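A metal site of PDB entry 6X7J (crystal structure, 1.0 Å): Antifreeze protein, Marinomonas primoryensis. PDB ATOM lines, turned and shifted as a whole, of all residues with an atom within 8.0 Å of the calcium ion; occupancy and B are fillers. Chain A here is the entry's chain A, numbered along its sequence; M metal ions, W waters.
The side-chain amide nitrogen (NE2) of Gln 59 lies close to the side-chain carboxylate (OD1) of Asp 72 (3.0 Å).
The backbone NH of Gly 55 is in hydrogen-bond range of the side-chain carboxylate of Asp 75, 2.8 Å away.
The calcium ion is bound by the backbone carbonyl oxygen of Pro 73 (2.3 Å), water W4 (2.4 Å), water W2 (2.4 Å), the backbone carbonyl oxygen of Gly 55 (2.4 Å), water W1 (2.4 Å), water W3 (2.4 Å) and the side-chain carboxylate of Asp 72 (2.5 Å).
The calcium ion has seven donor atoms within binding distance.
Water W1 bridges O of Gly 74 (2.8 Å) and O of Ala 53 (3.0 Å).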
ATOM      1  N   TYR A  12     -16.623  -3.502  24.250  1.00  0.00           N
ATOM      2  CA  TYR A  12     -17.348  -3.803  23.015  1.00  0.00           C
ATOM      3  C   TYR A  12     -18.549  -2.859  22.902  1.00  0.00           C
ATOM      4  O   TYR A  12     -19.276  -2.641  23.880  1.00  0.00           O
ATOM      5  CB  TYR A  12     -17.844  -5.241  23.027  1.00  0.00           C
ATOM      6  CG  TYR A  12     -18.809  -5.529  21.905  1.00  0.00           C
ATOM      7  CD1 TYR A  12     -18.372  -5.709  20.604  1.00  0.00           C
ATOM      8  CD2 TYR A  12     -20.184  -5.508  22.116  1.00  0.00           C
ATOM      9  CE1 TYR A  12     -19.250  -5.895  19.546  1.00  0.00           C
ATOM     10  CE2 TYR A  12     -21.081  -5.667  21.084  1.00  0.00           C
ATOM     11  CZ  TYR A  12     -20.612  -5.867  19.791  1.00  0.00           C
ATOM     12  OH  TYR A  12     -21.466  -6.011  18.717  1.00  0.00           O
ATOM     13  N   VAL A  52     -20.171  -9.727  13.282  1.00  0.00           N
ATOM     14  CA  VAL A  52     -19.648  -9.927  14.639  1.00  0.00           C
ATOM     15  C   VAL A  52     -20.699  -9.611  15.700  1.00  0.00           C
ATOM     16  O   VAL A  52     -20.650 -10.177  16.796  1.00  0.00           O
ATOM     17  CB  VAL A  52     -18.374  -9.118  14.905  1.00  0.00           C
ATOM     18  CG1 VAL A  52     -18.639  -7.671  15.323  1.00  0.00           C
ATOM     19  CG2 VAL A  52     -17.512  -9.813  15.977  1.00  0.00           C
ATOM     20  N   ALA A  53     -21.614  -8.688  15.387  1.00  0.00           N
ATOM     21  CA  ALA A  53     -22.536  -8.127  16.371  1.00  0.00           C
ATOM     22  C   ALA A  53     -23.803  -8.963  16.548  1.00  0.00           C
ATOM     23  O   ALA A  53     -24.631  -8.623  17.401  1.00  0.00           O
ATOM     24  CB  ALA A  53     -22.854  -6.691  15.986  1.00  0.00           C
ATOM     25  N   LYS A  54     -23.930 -10.050  15.783  1.00  0.00           N
ATOM     26  CA  LYS A  54     -25.114 -10.933  15.870  1.00  0.00           C
ATOM     27  C   LYS A  54     -24.837 -12.160  16.737  1.00  0.00           C
ATOM     28  O   LYS A  54     -23.748 -12.722  16.702  1.00  0.00           O
ATOM     29  CB  LYS A  54     -25.575 -11.323  14.469  1.00  0.00           C
ATOM     30  CG  LYS A  54     -25.899 -10.109  13.616  1.00  0.00           C
ATOM     31  CD  LYS A  54     -27.266 -10.050  13.059  1.00  0.00           C
ATOM     32  CE  LYS A  54     -27.565  -8.691  12.507  1.00  0.00           C
ATOM     33  NZ  LYS A  54     -28.730  -8.838  11.622  1.00  0.00           N
ATOM     34  N   GLY A  55     -25.874 -12.608  17.434  1.00  0.00           N
ATOM     35  CA  GLY A  55     -25.844 -13.901  18.130  1.00  0.00           C
ATOM     36  C   GLY A  55     -24.611 -14.020  19.028  1.00  0.00           C
ATOM     37  O   GLY A  55     -24.320 -13.121  19.789  1.00  0.00           O
ATOM     38  N   THR A  56     -23.957 -15.172  18.910  1.00  0.00           N
ATOM     39  CA  THR A  56     -22.767 -15.451  19.732  1.00  0.00           C
ATOM     40  C   THR A  56     -21.467 -15.253  18.931  1.00  0.00           C
ATOM     41  O   THR A  56     -20.416 -15.766  19.322  1.00  0.00           O
ATOM     42  CB  THR A  56     -22.834 -16.877  20.284  1.00  0.00           C
ATOM     43  OG1 THR A  56     -22.903 -17.839  19.216  1.00  0.00           O
ATOM     44  CG2 THR A  56     -24.055 -17.085  21.158  1.00  0.00           C
ATOM     45  N   HIS A  57     -21.537 -14.468  17.854  1.00  0.00           N
ATOM     46  CA  HIS A  57     -20.335 -14.275  17.040  1.00  0.00           C
ATOM     47  C   HIS A  57     -19.239 -13.551  17.811  1.00  0.00           C
ATOM     48  O   HIS A  57     -18.060 -13.839  17.593  1.00  0.00           O
ATOM     49  CB  HIS A  57     -20.704 -13.579  15.749  1.00  0.00           C
ATOM     50  CG  HIS A  57     -21.609 -14.418  14.909  1.00  0.00           C
ATOM     51  ND1 HIS A  57     -22.449 -13.868  13.953  1.00  0.00           N
ATOM     52  CD2 HIS A  57     -21.861 -15.742  14.902  1.00  0.00           C
ATOM     53  CE1 HIS A  57     -23.174 -14.831  13.418  1.00  0.00           C
ATOM     54  NE2 HIS A  57     -22.813 -15.979  13.946  1.00  0.00           N
ATOM     55  N   LEU A  58     -19.596 -12.600  18.685  1.00  0.00           N
ATOM     56  CA  LEU A  58     -18.564 -11.902  19.466  1.00  0.00           C
ATOM     57  C   LEU A  58     -17.812 -12.868  20.357  1.00  0.00           C
ATOM     58  O   LEU A  58     -16.583 -12.792  20.479  1.00  0.00           O
ATOM     59  CB  LEU A  58     -19.192 -10.789  20.281  1.00  0.00           C
ATOM     60  CG  LEU A  58     -18.221 -10.008  21.178  1.00  0.00           C
ATOM     61  CD1 LEU A  58     -17.201  -9.214  20.364  1.00  0.00           C
ATOM     62  CD2 LEU A  58     -18.990  -9.121  22.117  1.00  0.00           C
ATOM     63  N   GLN A  59     -18.554 -13.760  21.002  1.00  0.00           N
ATOM     64  CA  GLN A  59     -17.935 -14.778  21.884  1.00  0.00           C
ATOM     65  C   GLN A  59     -16.957 -15.624  21.078  1.00  0.00           C
ATOM     66  O   GLN A  59     -15.857 -15.938  21.554  1.00  0.00           O
ATOM     67  CB  GLN A  59     -19.029 -15.685  22.465  1.00  0.00           C
ATOM     68  CG  GLN A  59     -19.858 -15.097  23.573  1.00  0.00           C
ATOM     69  CD  GLN A  59     -20.956 -14.127  23.178  1.00  0.00           C
ATOM     70  OE1 GLN A  59     -21.165 -13.776  22.016  1.00  0.00           O
ATOM     71  NE2 GLN A  59     -21.708 -13.679  24.191  1.00  0.00           N
ATOM     72  N   LEU A  69     -16.202 -11.685  29.512  1.00  0.00           N
ATOM     73  CA  LEU A  69     -17.271 -10.753  29.139  1.00  0.00           C
ATOM     74  C   LEU A  69     -18.154 -10.452  30.343  1.00  0.00           C
ATOM     75  O   LEU A  69     -18.610 -11.350  31.069  1.00  0.00           O
ATOM     76  CB  LEU A  69     -18.134 -11.369  28.019  1.00  0.00           C
ATOM     77  CG  LEU A  69     -17.553 -11.212  26.624  1.00  0.00           C
ATOM     78  CD1 LEU A  69     -18.263 -12.167  25.678  1.00  0.00           C
ATOM     79  CD2 LEU A  69     -17.665  -9.792  26.109  1.00  0.00           C
ATOM     80  N   THR A  71     -21.213  -9.217  30.045  1.00  0.00           N
ATOM     81  CA  THR A  71     -22.582  -9.548  29.649  1.00  0.00           C
ATOM     82  C   THR A  71     -22.482 -10.131  28.255  1.00  0.00           C
ATOM     83  O   THR A  71     -21.445 -10.016  27.585  1.00  0.00           O
ATOM     84  CB  THR A  71     -23.440  -8.306  29.750  1.00  0.00           C
ATOM     85  OG1 THR A  71     -24.824  -8.657  29.736  1.00  0.00           O
ATOM     86  CG2 THR A  71     -23.084  -7.292  28.726  1.00  0.00           C
ATOM     87  N   ASP A  72     -23.592 -10.713  27.805  1.00  0.00           N
ATOM     88  CA  ASP A  72     -23.775 -11.169  26.402  1.00  0.00           C
ATOM     89  C   ASP A  72     -24.559 -10.087  25.696  1.00  0.00           C
ATOM     90  O   ASP A  72     -25.752  -9.915  25.938  1.00  0.00           O
ATOM     91  CB  ASP A  72     -24.523 -12.467  26.352  1.00  0.00           C
ATOM     92  CG  ASP A  72     -24.829 -12.989  24.965  1.00  0.00           C
ATOM     93  OD1 ASP A  72     -24.357 -12.349  23.982  1.00  0.00           O
ATOM     94  OD2 ASP A  72     -25.531 -14.018  24.868  1.00  0.00           O
ATOM     95  N   PRO A  73     -23.930  -9.252  24.858  1.00  0.00           N
ATOM     96  CA  PRO A  73     -24.662  -8.218  24.148  1.00  0.00           C
ATOM     97  C   PRO A  73     -25.825  -8.789  23.348  1.00  0.00           C
ATOM     98  O   PRO A  73     -25.761  -9.888  22.829  1.00  0.00           O
ATOM     99  CB  PRO A  73     -23.627  -7.589  23.183  1.00  0.00           C
ATOM    100  CG  PRO A  73     -22.275  -7.931  23.816  1.00  0.00           C
ATOM    101  CD  PRO A  73     -22.495  -9.275  24.442  1.00  0.00           C
ATOM    102  N   GLY A  74     -26.881  -7.973  23.194  1.00  0.00           N
ATOM    103  CA  GLY A  74     -27.933  -8.305  22.256  1.00  0.00           C
ATOM    104  C   GLY A  74     -27.453  -8.110  20.801  1.00  0.00           C
ATOM    105  O   GLY A  74     -26.313  -7.705  20.551  1.00  0.00           O
ATOM    106  N   ASP A  75     -28.324  -8.433  19.862  1.00  0.00           N
ATOM    107  CA  ASP A  75     -27.962  -8.306  18.451  1.00  0.00           C
ATOM    108  C   ASP A  75     -27.826  -6.831  18.078  1.00  0.00           C
ATOM    109  O   ASP A  75     -28.623  -5.975  18.487  1.00  0.00           O
ATOM    110  CB  ASP A  75     -29.024  -8.916  17.560  1.00  0.00           C
ATOM    111  CG  ASP A  75     -29.063 -10.432  17.497  1.00  0.00           C
ATOM    112  OD1 ASP A  75     -28.175 -11.089  18.085  1.00  0.00           O
ATOM    113  OD2 ASP A  75     -30.006 -10.935  16.837  1.00  0.00           O
ATOM    114  N   ASN A  76     -26.878  -6.605  17.179  1.00  0.00           N
ATOM    115  CA  ASN A  76     -26.724  -5.325  16.437  1.00  0.00           C
ATOM    116  C   ASN A  76     -26.264  -5.703  15.025  1.00  0.00           C
ATOM    117  O   ASN A  76     -25.814  -6.820  14.793  1.00  0.00           O
ATOM    118  CB  ASN A  76     -25.660  -4.317  17.112  1.00  0.00           C
ATOM    119  CG  ASN A  76     -26.308  -3.590  18.285  1.00  0.00           C
ATOM    120  OD1 ASN A  76     -27.227  -2.733  18.060  1.00  0.00           O
ATOM    121  ND2 ASN A  76     -25.792  -3.794  19.427  1.00  0.00           N
HETATM  122 CA    CA M   1     -25.046 -11.802  21.678  1.00  0.00          CA
HETATM  123  O   HOH W   1     -24.696  -9.976  20.128  1.00  0.00           O
HETATM  124  O   HOH W   2     -27.204 -11.706  20.646  1.00  0.00           O
HETATM  125  O   HOH W   3     -22.642 -11.467  21.605  1.00  0.00           O
HETATM  126  O   HOH W   4     -25.925 -13.946  22.180  1.00  0.00           O
